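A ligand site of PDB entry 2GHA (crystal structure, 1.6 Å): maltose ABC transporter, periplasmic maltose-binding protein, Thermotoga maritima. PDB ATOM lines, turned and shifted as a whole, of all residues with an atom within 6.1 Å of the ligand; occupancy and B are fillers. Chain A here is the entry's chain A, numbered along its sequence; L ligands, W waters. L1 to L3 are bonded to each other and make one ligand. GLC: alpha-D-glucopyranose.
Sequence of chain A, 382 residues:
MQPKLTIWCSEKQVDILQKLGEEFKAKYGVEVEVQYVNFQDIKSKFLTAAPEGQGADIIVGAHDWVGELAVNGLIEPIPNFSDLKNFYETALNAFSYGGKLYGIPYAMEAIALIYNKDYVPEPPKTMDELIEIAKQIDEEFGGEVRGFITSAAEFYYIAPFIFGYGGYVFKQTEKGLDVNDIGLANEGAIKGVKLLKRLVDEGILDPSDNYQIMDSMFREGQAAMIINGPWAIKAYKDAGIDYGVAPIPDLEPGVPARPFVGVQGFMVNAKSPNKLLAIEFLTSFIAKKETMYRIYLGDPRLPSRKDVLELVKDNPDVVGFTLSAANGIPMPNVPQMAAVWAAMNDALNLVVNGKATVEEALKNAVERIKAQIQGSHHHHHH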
ATOM      1  N   SER A  10      22.624  28.334 -17.521  1.00  0.00           N
ATOM      2  CA  SER A  10      22.824  27.249 -18.466  1.00  0.00           C
ATOM      3  C   SER A  10      22.371  27.651 -19.870  1.00  0.00           C
ATOM      4  O   SER A  10      21.750  28.699 -20.061  1.00  0.00           O
ATOM      5  CB  SER A  10      22.053  26.024 -17.997  1.00  0.00           C
ATOM      6  OG  SER A  10      20.711  26.042 -18.463  1.00  0.00           O
ATOM      7  N   GLU A  11      22.634  26.814 -20.855  1.00  0.00           N
ATOM      8  CA  GLU A  11      22.203  27.096 -22.219  1.00  0.00           C
ATOM      9  C   GLU A  11      20.675  27.298 -22.367  1.00  0.00           C
ATOM     10  O   GLU A  11      20.241  28.029 -23.276  1.00  0.00           O
ATOM     11  CB  GLU A  11      22.671  25.992 -23.170  1.00  0.00           C
ATOM     12  CG  GLU A  11      22.002  24.657 -22.945  1.00  0.00           C
ATOM     13  CD  GLU A  11      22.607  23.911 -21.797  1.00  0.00           C
ATOM     14  OE1 GLU A  11      23.747  24.245 -21.407  1.00  0.00           O
ATOM     15  OE2 GLU A  11      21.931  22.970 -21.293  1.00  0.00           O
ATOM     16  N   LYS A  12      19.876  26.703 -21.482  1.00  0.00           N
ATOM     17  CA  LYS A  12      18.433  26.627 -21.654  1.00  0.00           C
ATOM     18  C   LYS A  12      17.789  28.015 -21.488  1.00  0.00           C
ATOM     19  O   LYS A  12      16.777  28.311 -22.104  1.00  0.00           O
ATOM     20  CB  LYS A  12      17.793  25.652 -20.661  1.00  0.00           C
ATOM     21  CG  LYS A  12      18.305  24.251 -20.805  1.00  0.00           C
ATOM     22  CD  LYS A  12      18.057  23.605 -22.178  1.00  0.00           C
ATOM     23  CE  LYS A  12      18.531  22.143 -22.184  1.00  0.00           C
ATOM     24  NZ  LYS A  12      18.071  21.445 -23.430  1.00  0.00           N
ATOM     25  N   GLN A  13      18.386  28.855 -20.665  1.00  0.00           N
ATOM     26  CA  GLN A  13      17.780  30.161 -20.315  1.00  0.00           C
ATOM     27  C   GLN A  13      18.345  31.347 -21.075  1.00  0.00           C
ATOM     28  O   GLN A  13      17.781  32.459 -21.018  1.00  0.00           O
ATOM     29  CB  GLN A  13      17.869  30.465 -18.819  1.00  0.00           C
ATOM     30  CG  GLN A  13      17.277  29.406 -17.904  1.00  0.00           C
ATOM     31  CD  GLN A  13      18.270  28.360 -17.439  1.00  0.00           C
ATOM     32  OE1 GLN A  13      19.389  28.251 -17.955  1.00  0.00           O
ATOM     33  NE2 GLN A  13      17.857  27.579 -16.480  1.00  0.00           N
ATOM     34  N   ASN A  38      28.120  26.241 -18.399  1.00  0.00           N
ATOM     35  CA  ASN A  38      27.557  24.891 -18.292  1.00  0.00           C
ATOM     36  C   ASN A  38      26.997  24.716 -16.881  1.00  0.00           C
ATOM     37  O   ASN A  38      27.645  25.081 -15.886  1.00  0.00           O
ATOM     38  CB  ASN A  38      28.612  23.808 -18.582  1.00  0.00           C
ATOM     39  CG  ASN A  38      28.002  22.390 -18.651  1.00  0.00           C
ATOM     40  OD1 ASN A  38      27.556  21.830 -17.641  1.00  0.00           O
ATOM     41  ND2 ASN A  38      27.953  21.835 -19.849  1.00  0.00           N
ATOM     42  N   PHE A  39      25.793  24.188 -16.807  1.00  0.00           N
ATOM     43  CA  PHE A  39      25.096  24.058 -15.505  1.00  0.00           C
ATOM     44  C   PHE A  39      25.967  23.404 -14.431  1.00  0.00           C
ATOM     45  O   PHE A  39      25.984  23.848 -13.276  1.00  0.00           O
ATOM     46  CB  PHE A  39      23.817  23.269 -15.674  1.00  0.00           C
ATOM     47  CG  PHE A  39      23.099  23.048 -14.384  1.00  0.00           C
ATOM     48  CD1 PHE A  39      22.246  23.995 -13.903  1.00  0.00           C
ATOM     49  CD2 PHE A  39      23.364  21.912 -13.606  1.00  0.00           C
ATOM     50  CE1 PHE A  39      21.613  23.810 -12.692  1.00  0.00           C
ATOM     51  CE2 PHE A  39      22.748  21.746 -12.376  1.00  0.00           C
ATOM     52  CZ  PHE A  39      21.880  22.693 -11.939  1.00  0.00           C
ATOM     53  N   GLN A  40      26.687  22.359 -14.811  1.00  0.00           N
ATOM     54  CA  GLN A  40      27.530  21.594 -13.893  1.00  0.00           C
ATOM     55  C   GLN A  40      28.733  22.391 -13.365  1.00  0.00           C
ATOM     56  O   GLN A  40      29.389  21.959 -12.430  1.00  0.00           O
ATOM     57  CB  GLN A  40      28.004  20.277 -14.555  1.00  0.00           C
ATOM     58  CG  GLN A  40      26.986  19.494 -15.434  1.00  0.00           C
ATOM     59  CD  GLN A  40      25.707  19.046 -14.738  1.00  0.00           C
ATOM     60  OE1 GLN A  40      25.692  18.689 -13.550  1.00  0.00           O
ATOM     61  NE2 GLN A  40      24.618  18.984 -15.524  1.00  0.00           N
ATOM     62  N   LYS A  43      28.057  26.532  -9.981  1.00  0.00           N
ATOM     63  CA  LYS A  43      28.230  26.757  -8.543  1.00  0.00           C
ATOM     64  C   LYS A  43      29.727  26.787  -8.217  1.00  0.00           C
ATOM     65  O   LYS A  43      30.170  27.642  -7.430  1.00  0.00           O
ATOM     66  CB  LYS A  43      27.526  25.665  -7.725  1.00  0.00           C
ATOM     67  CG  LYS A  43      27.803  25.802  -6.237  1.00  0.00           C
ATOM     68  CD  LYS A  43      26.740  25.175  -5.354  1.00  0.00           C
ATOM     69  CE  LYS A  43      26.606  23.662  -5.562  1.00  0.00           C
ATOM     70  NZ  LYS A  43      27.810  22.889  -5.124  1.00  0.00           N
ATOM     71  N   ALA A  62      19.737  25.620  -9.391  1.00  0.00           N
ATOM     72  CA  ALA A  62      18.892  24.746  -8.578  1.00  0.00           C
ATOM     73  C   ALA A  62      18.927  25.053  -7.087  1.00  0.00           C
ATOM     74  O   ALA A  62      19.945  25.505  -6.536  1.00  0.00           O
ATOM     75  CB  ALA A  62      19.287  23.266  -8.838  1.00  0.00           C
ATOM     76  N   HIS A  63      17.831  24.777  -6.406  1.00  0.00           N
ATOM     77  CA  HIS A  63      17.674  25.192  -5.030  1.00  0.00           C
ATOM     78  C   HIS A  63      18.584  24.439  -4.058  1.00  0.00           C
ATOM     79  O   HIS A  63      18.800  24.901  -2.931  1.00  0.00           O
ATOM     80  CB  HIS A  63      16.214  25.046  -4.584  1.00  0.00           C
ATOM     81  CG  HIS A  63      15.848  23.634  -4.245  1.00  0.00           C
ATOM     82  ND1 HIS A  63      15.391  22.743  -5.177  1.00  0.00           N
ATOM     83  CD2 HIS A  63      15.850  22.975  -3.065  1.00  0.00           C
ATOM     84  CE1 HIS A  63      15.155  21.578  -4.595  1.00  0.00           C
ATOM     85  NE2 HIS A  63      15.448  21.685  -3.317  1.00  0.00           N
ATOM     86  N   ASP A  64      19.100  23.284  -4.453  1.00  0.00           N
ATOM     87  CA  ASP A  64      19.971  22.527  -3.526  1.00  0.00           C
ATOM     88  C   ASP A  64      21.231  23.316  -3.188  1.00  0.00           C
ATOM     89  O   ASP A  64      21.904  23.044  -2.184  1.00  0.00           O
ATOM     90  CB  ASP A  64      20.344  21.130  -4.063  1.00  0.00           C
ATOM     91  CG  ASP A  64      21.072  21.175  -5.411  1.00  0.00           C
ATOM     92  OD1 ASP A  64      20.444  21.621  -6.391  1.00  0.00           O
ATOM     93  OD2 ASP A  64      22.232  20.735  -5.480  1.00  0.00           O
ATOM     94  N   TRP A  65      21.592  24.294  -4.026  1.00  0.00           N
ATOM     95  CA  TRP A  65      22.786  25.107  -3.777  1.00  0.00           C
ATOM     96  C   TRP A  65      22.657  26.060  -2.606  1.00  0.00           C
ATOM     97  O   TRP A  65      23.666  26.596  -2.116  1.00  0.00           O
ATOM     98  CB  TRP A  65      23.106  25.980  -5.004  1.00  0.00           C
ATOM     99  CG  TRP A  65      23.249  25.293  -6.319  1.00  0.00           C
ATOM    100  CD1 TRP A  65      23.268  23.946  -6.576  1.00  0.00           C
ATOM    101  CD2 TRP A  65      23.438  25.937  -7.601  1.00  0.00           C
ATOM    102  NE1 TRP A  65      23.450  23.725  -7.907  1.00  0.00           N
ATOM    103  CE2 TRP A  65      23.523  24.919  -8.568  1.00  0.00           C
ATOM    104  CE3 TRP A  65      23.502  27.288  -8.021  1.00  0.00           C
ATOM    105  CZ2 TRP A  65      23.700  25.193  -9.927  1.00  0.00           C
ATOM    106  CZ3 TRP A  65      23.646  27.555  -9.376  1.00  0.00           C
ATOM    107  CH2 TRP A  65      23.737  26.516 -10.307  1.00  0.00           C
ATOM    108  N   TYR A 106      11.597  30.287 -10.581  1.00  0.00           N
ATOM    109  CA  TYR A 106      10.773  30.387 -11.793  1.00  0.00           C
ATOM    110  C   TYR A 106      10.051  29.087 -12.161  1.00  0.00           C
ATOM    111  O   TYR A 106       9.056  29.113 -12.903  1.00  0.00           O
ATOM    112  CB  TYR A 106      11.531  30.950 -13.000  1.00  0.00           C
ATOM    113  CG  TYR A 106      12.495  30.013 -13.714  1.00  0.00           C
ATOM    114  CD1 TYR A 106      12.046  29.162 -14.686  1.00  0.00           C
ATOM    115  CD2 TYR A 106      13.851  30.003 -13.420  1.00  0.00           C
ATOM    116  CE1 TYR A 106      12.917  28.320 -15.349  1.00  0.00           C
ATOM    117  CE2 TYR A 106      14.724  29.143 -14.072  1.00  0.00           C
ATOM    118  CZ  TYR A 106      14.245  28.302 -15.063  1.00  0.00           C
ATOM    119  OH  TYR A 106      15.092  27.427 -15.746  1.00  0.00           O
ATOM    120  N   GLU A 109      10.520  21.037 -11.147  1.00  0.00           N
ATOM    121  CA  GLU A 109      10.859  20.012 -12.133  1.00  0.00           C
ATOM    122  C   GLU A 109      11.115  18.689 -11.447  1.00  0.00           C
ATOM    123  O   GLU A 109      11.415  18.628 -10.267  1.00  0.00           O
ATOM    124  CB  GLU A 109      12.109  20.415 -12.902  1.00  0.00           C
ATOM    125  CG  GLU A 109      13.377  20.478 -12.050  1.00  0.00           C
ATOM    126  CD  GLU A 109      14.524  21.209 -12.695  1.00  0.00           C
ATOM    127  OE1 GLU A 109      14.282  21.839 -13.740  1.00  0.00           O
ATOM    128  OE2 GLU A 109      15.633  21.147 -12.113  1.00  0.00           O
ATOM    129  N   GLU A 154      25.097   8.491 -12.759  1.00  0.00           N
ATOM    130  CA  GLU A 154      24.893   9.807 -12.164  1.00  0.00           C
ATOM    131  C   GLU A 154      23.736   9.676 -11.152  1.00  0.00           C
ATOM    132  O   GLU A 154      22.596   9.372 -11.524  1.00  0.00           O
ATOM    133  CB  GLU A 154      24.595  10.796 -13.283  1.00  0.00           C
ATOM    134  CG  GLU A 154      24.676  12.236 -12.911  1.00  0.00           C
ATOM    135  CD  GLU A 154      24.461  13.201 -14.073  1.00  0.00           C
ATOM    136  OE1 GLU A 154      24.472  12.784 -15.267  1.00  0.00           O
ATOM    137  OE2 GLU A 154      24.345  14.418 -13.797  1.00  0.00           O
ATOM    138  N   PHE A 155      24.054   9.848  -9.874  1.00  0.00           N
ATOM    139  CA  PHE A 155      23.085   9.677  -8.788  1.00  0.00           C
ATOM    140  C   PHE A 155      21.750  10.405  -8.987  1.00  0.00           C
ATOM    141  O   PHE A 155      20.693   9.847  -8.741  1.00  0.00           O
ATOM    142  CB  PHE A 155      23.728  10.043  -7.446  1.00  0.00           C
ATOM    143  CG  PHE A 155      22.771  10.120  -6.282  1.00  0.00           C
ATOM    144  CD1 PHE A 155      21.937   9.060  -5.964  1.00  0.00           C
ATOM    145  CD2 PHE A 155      22.712  11.264  -5.490  1.00  0.00           C
ATOM    146  CE1 PHE A 155      21.073   9.134  -4.834  1.00  0.00           C
ATOM    147  CE2 PHE A 155      21.836  11.349  -4.411  1.00  0.00           C
ATOM    148  CZ  PHE A 155      21.012  10.279  -4.103  1.00  0.00           C
ATOM    149  N   TYR A 156      21.801  11.644  -9.419  1.00  0.00           N
ATOM    150  CA  TYR A 156      20.578  12.417  -9.689  1.00  0.00           C
ATOM    151  C   TYR A 156      19.555  11.629 -10.539  1.00  0.00           C
ATOM    152  O   TYR A 156      18.362  11.650 -10.237  1.00  0.00           O
ATOM    153  CB  TYR A 156      20.912  13.755 -10.342  1.00  0.00           C
ATOM    154  CG  TYR A 156      19.701  14.622 -10.612  1.00  0.00           C
ATOM    155  CD1 TYR A 156      19.159  15.452  -9.637  1.00  0.00           C
ATOM    156  CD2 TYR A 156      19.004  14.528 -11.828  1.00  0.00           C
ATOM    157  CE1 TYR A 156      18.049  16.201  -9.863  1.00  0.00           C
ATOM    158  CE2 TYR A 156      17.888  15.292 -12.072  1.00  0.00           C
ATOM    159  CZ  TYR A 156      17.393  16.135 -11.074  1.00  0.00           C
ATOM    160  OH  TYR A 156      16.256  16.882 -11.325  1.00  0.00           O
ATOM    161  N   TYR A 157      20.033  10.922 -11.576  1.00  0.00           N
ATOM    162  CA  TYR A 157      19.179  10.152 -12.503  1.00  0.00           C
ATOM    163  C   TYR A 157      18.790   8.755 -12.015  1.00  0.00           C
ATOM    164  O   TYR A 157      17.768   8.218 -12.488  1.00  0.00           O
ATOM    165  CB  TYR A 157      19.838  10.051 -13.895  1.00  0.00           C
ATOM    166  CG  TYR A 157      19.897  11.398 -14.520  1.00  0.00           C
ATOM    167  CD1 TYR A 157      18.838  11.892 -15.263  1.00  0.00           C
ATOM    168  CD2 TYR A 157      20.984  12.252 -14.316  1.00  0.00           C
ATOM    169  CE1 TYR A 157      18.883  13.195 -15.781  1.00  0.00           C
ATOM    170  CE2 TYR A 157      21.031  13.541 -14.839  1.00  0.00           C
ATOM    171  CZ  TYR A 157      19.977  14.014 -15.547  1.00  0.00           C
ATOM    172  OH  TYR A 157      20.035  15.294 -16.081  1.00  0.00           O
ATOM    173  N   TYR A 211      24.729  11.885 -19.707  1.00  0.00           N
ATOM    174  CA  TYR A 211      23.718  12.857 -20.108  1.00  0.00           C
ATOM    175  C   TYR A 211      23.784  13.197 -21.601  1.00  0.00           C
ATOM    176  O   TYR A 211      22.761  13.172 -22.300  1.00  0.00           O
ATOM    177  CB  TYR A 211      23.814  14.147 -19.255  1.00  0.00           C
ATOM    178  CG  TYR A 211      22.647  15.017 -19.593  1.00  0.00           C
ATOM    179  CD1 TYR A 211      21.448  14.853 -18.904  1.00  0.00           C
ATOM    180  CD2 TYR A 211      22.705  15.942 -20.626  1.00  0.00           C
ATOM    181  CE1 TYR A 211      20.335  15.567 -19.255  1.00  0.00           C
ATOM    182  CE2 TYR A 211      21.574  16.669 -20.978  1.00  0.00           C
ATOM    183  CZ  TYR A 211      20.404  16.470 -20.266  1.00  0.00           C
ATOM    184  OH  TYR A 211      19.276  17.177 -20.607  1.00  0.00           O
ATOM    185  N   ASN A 228      14.629  11.736 -18.239  1.00  0.00           N
ATOM    186  CA  ASN A 228      15.182  13.096 -18.298  1.00  0.00           C
ATOM    187  C   ASN A 228      14.095  14.074 -17.869  1.00  0.00           C
ATOM    188  O   ASN A 228      12.946  13.679 -17.663  1.00  0.00           O
ATOM    189  CB  ASN A 228      15.690  13.407 -19.723  1.00  0.00           C
ATOM    190  CG  ASN A 228      16.760  14.508 -19.762  1.00  0.00           C
ATOM    191  OD1 ASN A 228      17.143  15.069 -18.723  1.00  0.00           O
ATOM    192  ND2 ASN A 228      17.233  14.831 -20.959  1.00  0.00           N
ATOM    193  N   TRP A 231      13.636  20.366 -18.825  1.00  0.00           N
ATOM    194  CA  TRP A 231      14.645  21.196 -19.465  1.00  0.00           C
ATOM    195  C   TRP A 231      15.052  20.732 -20.834  1.00  0.00           C
ATOM    196  O   TRP A 231      15.606  21.522 -21.607  1.00  0.00           O
ATOM    197  CB  TRP A 231      15.931  21.308 -18.613  1.00  0.00           C
ATOM    198  CG  TRP A 231      16.497  20.032 -18.237  1.00  0.00           C
ATOM    199  CD1 TRP A 231      17.295  19.261 -18.989  1.00  0.00           C
ATOM    200  CD2 TRP A 231      16.246  19.301 -17.050  1.00  0.00           C
ATOM    201  NE1 TRP A 231      17.619  18.092 -18.338  1.00  0.00           N
ATOM    202  CE2 TRP A 231      16.964  18.095 -17.121  1.00  0.00           C
ATOM    203  CE3 TRP A 231      15.498  19.572 -15.888  1.00  0.00           C
ATOM    204  CZ2 TRP A 231      16.952  17.128 -16.080  1.00  0.00           C
ATOM    205  CZ3 TRP A 231      15.475  18.609 -14.882  1.00  0.00           C
ATOM    206  CH2 TRP A 231      16.216  17.413 -14.969  1.00  0.00           C
ATOM    207  N   GLY A 262      13.274  19.334  -8.074  1.00  0.00           N
ATOM    208  CA  GLY A 262      14.125  20.509  -8.037  1.00  0.00           C
ATOM    209  C   GLY A 262      13.345  21.771  -8.284  1.00  0.00           C
ATOM    210  O   GLY A 262      12.329  21.756  -8.967  1.00  0.00           O
ATOM    211  N   GLN A 264      14.143  25.675  -9.785  1.00  0.00           N
ATOM    212  CA  GLN A 264      15.133  26.513 -10.472  1.00  0.00           C
ATOM    213  C   GLN A 264      14.802  27.963 -10.169  1.00  0.00           C
ATOM    214  O   GLN A 264      13.633  28.345 -10.109  1.00  0.00           O
ATOM    215  CB  GLN A 264      15.051  26.341 -11.990  1.00  0.00           C
ATOM    216  CG  GLN A 264      15.502  24.933 -12.452  1.00  0.00           C
ATOM    217  CD  GLN A 264      16.999  24.713 -12.404  1.00  0.00           C
ATOM    218  OE1 GLN A 264      17.793  25.614 -12.610  1.00  0.00           O
ATOM    219  NE2 GLN A 264      17.395  23.469 -12.118  1.00  0.00           N
ATOM    220  N   ASP A 299      11.724  28.176 -21.887  1.00  0.00           N
ATOM    221  CA  ASP A 299      12.371  27.103 -21.098  1.00  0.00           C
ATOM    222  C   ASP A 299      11.270  26.434 -20.262  1.00  0.00           C
ATOM    223  O   ASP A 299      11.138  26.687 -19.068  1.00  0.00           O
ATOM    224  CB  ASP A 299      13.512  27.693 -20.248  1.00  0.00           C
ATOM    225  CG  ASP A 299      14.116  26.708 -19.274  1.00  0.00           C
ATOM    226  OD1 ASP A 299      14.001  25.484 -19.505  1.00  0.00           O
ATOM    227  OD2 ASP A 299      14.705  27.163 -18.275  1.00  0.00           O
ATOM    228  N   ARG A 301       9.228  24.322 -18.003  1.00  0.00           N
ATOM    229  CA  ARG A 301       9.275  23.358 -16.888  1.00  0.00           C
ATOM    230  C   ARG A 301       7.925  23.416 -16.177  1.00  0.00           C
ATOM    231  O   ARG A 301       6.883  23.410 -16.856  1.00  0.00           O
ATOM    232  CB  ARG A 301      10.473  23.644 -15.984  1.00  0.00           C
ATOM    233  CG  ARG A 301      11.750  23.693 -16.819  1.00  0.00           C
ATOM    234  CD  ARG A 301      13.011  23.919 -15.952  1.00  0.00           C
ATOM    235  NE  ARG A 301      14.108  24.324 -16.824  1.00  0.00           N
ATOM    236  CZ  ARG A 301      15.413  24.154 -16.572  1.00  0.00           C
ATOM    237  NH1 ARG A 301      15.874  23.444 -15.551  1.00  0.00           N
ATOM    238  NH2 ARG A 301      16.293  24.615 -17.456  1.00  0.00           N
ATOM    239  N   MET A 331      15.026  17.890  -3.362  1.00  0.00           N
ATOM    240  CA  MET A 331      16.389  17.828  -2.952  1.00  0.00           C
ATOM    241  C   MET A 331      16.570  18.623  -1.668  1.00  0.00           C
ATOM    242  O   MET A 331      16.032  19.707  -1.530  1.00  0.00           O
ATOM    243  CB  MET A 331      17.331  18.445  -3.992  1.00  0.00           C
ATOM    244  CG  MET A 331      17.407  17.672  -5.289  1.00  0.00           C
ATOM    245  SD  MET A 331      18.591  18.379  -6.404  1.00  0.00           S
ATOM    246  CE  MET A 331      17.699  19.800  -7.002  1.00  0.00           C
ATOM    247  N   TRP A 341      26.923  14.250  -3.802  1.00  0.00           N
ATOM    248  CA  TRP A 341      26.791  13.936  -5.213  1.00  0.00           C
ATOM    249  C   TRP A 341      27.990  13.163  -5.749  1.00  0.00           C
ATOM    250  O   TRP A 341      27.823  12.163  -6.431  1.00  0.00           O
ATOM    251  CB  TRP A 341      26.610  15.194  -6.037  1.00  0.00           C
ATOM    252  CG  TRP A 341      25.437  16.050  -5.624  1.00  0.00           C
ATOM    253  CD1 TRP A 341      25.517  17.236  -4.960  1.00  0.00           C
ATOM    254  CD2 TRP A 341      24.032  15.801  -5.827  1.00  0.00           C
ATOM    255  NE1 TRP A 341      24.262  17.766  -4.785  1.00  0.00           N
ATOM    256  CE2 TRP A 341      23.331  16.912  -5.297  1.00  0.00           C
ATOM    257  CE3 TRP A 341      23.313  14.770  -6.412  1.00  0.00           C
ATOM    258  CZ2 TRP A 341      21.945  17.018  -5.342  1.00  0.00           C
ATOM    259  CZ3 TRP A 341      21.932  14.868  -6.454  1.00  0.00           C
ATOM    260  CH2 TRP A 341      21.263  15.986  -5.928  1.00  0.00           C
ATOM    261  N   ASN A 345      27.970   9.387  -7.296  1.00  0.00           N
ATOM    262  CA  ASN A 345      28.341   9.250  -8.690  1.00  0.00           C
ATOM    263  C   ASN A 345      29.484   8.231  -8.819  1.00  0.00           C
ATOM    264  O   ASN A 345      29.496   7.388  -9.691  1.00  0.00           O
ATOM    265  CB  ASN A 345      28.820  10.565  -9.286  1.00  0.00           C
ATOM    266  CG  ASN A 345      27.698  11.602  -9.485  1.00  0.00           C
ATOM    267  OD1 ASN A 345      26.504  11.261  -9.492  1.00  0.00           O
ATOM    268  ND2 ASN A 345      28.094  12.854  -9.701  1.00  0.00           N
HETATM  269  C1  GLC L   1      20.587  22.216 -18.432  1.00  0.00           C
HETATM  270  C2  GLC L   1      19.461  22.584 -17.467  1.00  0.00           C
HETATM  271  C3  GLC L   1      19.707  22.074 -16.065  1.00  0.00           C
HETATM  272  C4  GLC L   1      19.923  20.579 -16.086  1.00  0.00           C
HETATM  273  C5  GLC L   1      21.095  20.286 -17.028  1.00  0.00           C
HETATM  274  C6  GLC L   1      21.321  18.788 -17.212  1.00  0.00           C
HETATM  275  O1  GLC L   1      21.717  22.911 -18.024  1.00  0.00           O
HETATM  276  O2  GLC L   1      19.248  23.992 -17.418  1.00  0.00           O
HETATM  277  O3  GLC L   1      18.550  22.387 -15.263  1.00  0.00           O
HETATM  278  O4  GLC L   1      20.186  20.094 -14.779  1.00  0.00           O
HETATM  279  O5  GLC L   1      20.805  20.818 -18.328  1.00  0.00           O
HETATM  280  O6  GLC L   1      22.595  18.560 -17.814  1.00  0.00           O
HETATM  281  C1  GLC L   2      19.360  19.043 -14.285  1.00  0.00           C
HETATM  282  C2  GLC L   2      18.667  19.514 -13.007  1.00  0.00           C
HETATM  283  C3  GLC L   2      19.682  19.725 -11.888  1.00  0.00           C
HETATM  284  C4  GLC L   2      20.564  18.494 -11.736  1.00  0.00           C
HETATM  285  C5  GLC L   2      21.196  18.088 -13.067  1.00  0.00           C
HETATM  286  C6  GLC L   2      21.972  16.792 -12.908  1.00  0.00           C
HETATM  287  O2  GLC L   2      17.996  20.736 -13.247  1.00  0.00           O
HETATM  288  O3  GLC L   2      19.055  20.080 -10.639  1.00  0.00           O
HETATM  289  O4  GLC L   2      21.608  18.812 -10.817  1.00  0.00           O
HETATM  290  O5  GLC L   2      20.179  17.890 -14.045  1.00  0.00           O
HETATM  291  O6  GLC L   2      22.915  16.639 -13.984  1.00  0.00           O
HETATM  292  C1  GLC L   3      21.514  18.305  -9.494  1.00  0.00           C
HETATM  293  C2  GLC L   3      21.862  19.439  -8.521  1.00  0.00           C
HETATM  294  C3  GLC L   3      23.327  19.853  -8.651  1.00  0.00           C
HETATM  295  C4  GLC L   3      24.222  18.623  -8.518  1.00  0.00           C
HETATM  296  C5  GLC L   3      23.827  17.543  -9.531  1.00  0.00           C
HETATM  297  C6  GLC L   3      24.721  16.302  -9.427  1.00  0.00           C
HETATM  298  O2  GLC L   3      20.965  20.553  -8.731  1.00  0.00           O
HETATM  299  O3  GLC L   3      23.699  20.856  -7.705  1.00  0.00           O
HETATM  300  O4  GLC L   3      25.570  19.050  -8.746  1.00  0.00           O
HETATM  301  O5  GLC L   3      22.432  17.190  -9.391  1.00  0.00           O
HETATM  302  O6  GLC L   3      24.462  15.381 -10.479  1.00  0.00           O
HETATM  303  O   HOH W   1      26.380  19.538 -11.200  1.00  0.00           O
HETATM  304  O   HOH W   2      19.341  25.613 -14.803  1.00  0.00           O
HETATM  305  O   HOH W   3      27.966  18.553  -7.557  1.00  0.00           O
HETATM  306  O   HOH W   4      24.298  12.912  -9.313  1.00  0.00           O
HETATM  307  O   HOH W   5      22.764  16.184 -16.499  1.00  0.00           O
HETATM  308  O   HOH W   6      21.694  20.510 -21.300  1.00  0.00           O
HETATM  309  O   HOH W   7      26.251  22.054  -8.738  1.00  0.00           O
HETATM  310  O   HOH W   8      25.654  16.145 -12.707  1.00  0.00           O
HETATM  311  O   HOH W   9      16.357  19.253 -10.308  1.00  0.00           O
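The side-chain carboxylate (OE2) of Glu 154 sits at hydrogen-bond distance from an oxygen (O6) of GLC L2 (2.6 Å). The side-chain hydroxyl of Ser 10 sits at hydrogen-bond distance from an oxygen (O2) of GLC L1 (2.7 Å). An oxygen (O6) of GLC L1 is in hydrogen-bond range of the side-chain amide nitrogen (NE2) of Gln 40 (3.1 Å). An oxygen (O2) of GLC L2 sits at hydrogen-bond distance from the side-chain amide nitrogen (NE2) of Gln 264 (3.0 Å). The side-chain hydroxyl of Tyr 157 is in hydrogen-bond range of an oxygen (O5) of GLC L2, at 3.3 Å. O2 of GLC L3 sits at hydrogen-bond distance from OD1 of Asp 64. The indole nitrogen (NE1) of Trp 65 sits at hydrogen-bond distance from an oxygen (O3) of GLC L3 (2.9 Å). The guanidinium group (NH1) of Arg 301 sits at hydrogen-bond distance from an oxygen (O3) of GLC L1 (2.9 Å). The side-chain carboxylate (OE2) of Glu 109 lies within hydrogen-bond range of an oxygen (O2) of GLC L2 (2.7 Å). The side-chain carboxylate (OE2) of Glu 11 lies close to an oxygen (O1) of GLC L1.
The backbone carbonyl oxygen (O) of Gly 262 is in hydrogen-bond range of the backbone NH (N) of Glu 109 (2.9 Å). The backbone carbonyl oxygen (O) of Gln 264 lies within hydrogen-bond range of the backbone NH (N) of Tyr 106, 2.9 Å away. NE1 of Trp 231 is in hydrogen-bond range of OD1 of Asn 228, at 3.1 Å. The guanidinium group (NH2) of Arg 301 sits close to the side-chain amide nitrogen (NE2) of Gln 13, 3.5 Å away. The side-chain amide nitrogen (NE2) of Gln 264 is in hydrogen-bond range of the side-chain carboxylate (OE2) of Glu 109 (2.9 Å). The backbone NH (N) of Lys 12 lies close to the side-chain hydroxyl (OG) of Ser 10. NH1 of Arg 301 is in salt-bridge range of OE1 of Glu 109 (2.9 Å). The side-chain hydroxyl of Tyr 106 lies close to the guanidinium group of Arg 301 (3.4 Å).
Residues that only touch the ligand: Lys 12, Gln 13, Phe 39, Ala 62, Tyr 156, Tyr 211, Trp 231, Met 331 and Trp 341. Hydrophobic or aromatic side chains within 4 Å of the ligand: Phe 39, Ala 62, Trp 65, Tyr 156, Tyr 157, Tyr 211, Trp 231, Met 331 and Trp 341. Of the 28 residues printed, 19 come within 4 Å of the ligand.
Water W5 lies within hydrogen-bond range of O6 of GLC L2 (2.6 Å), OH of Tyr 157 (2.9 Å) and NE2 of Gln 40 (3.5 Å). Water W1 bridges OE1 of Gln 40 and O4 of GLC L3. Water W8 lies within hydrogen-bond range of the side-chain carboxylate of Glu 154 (2.4 Å), an oxygen (O6) of GLC L3 (2.6 Å) and the side-chain amide oxygen of Gln 40 (2.7 Å). Water W4 lies within hydrogen-bond range of an oxygen (O6) of GLC L3 (2.7 Å), the side-chain amide oxygen of Asn 345 (2.8 Å), the backbone NH of Tyr 156 (2.8 Å) and the backbone NH of Phe 155 (3.1 Å). Water W9 lies within hydrogen-bond range of OH of Tyr 156 (2.6 Å), OE2 of Glu 109 (2.7 Å) and O3 of GLC L2 (2.8 Å). Water W7 bridges an oxygen (O3) of GLC L3 (3.0 Å) and the indole nitrogen (NE1) of Trp 65 (3.4 Å).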
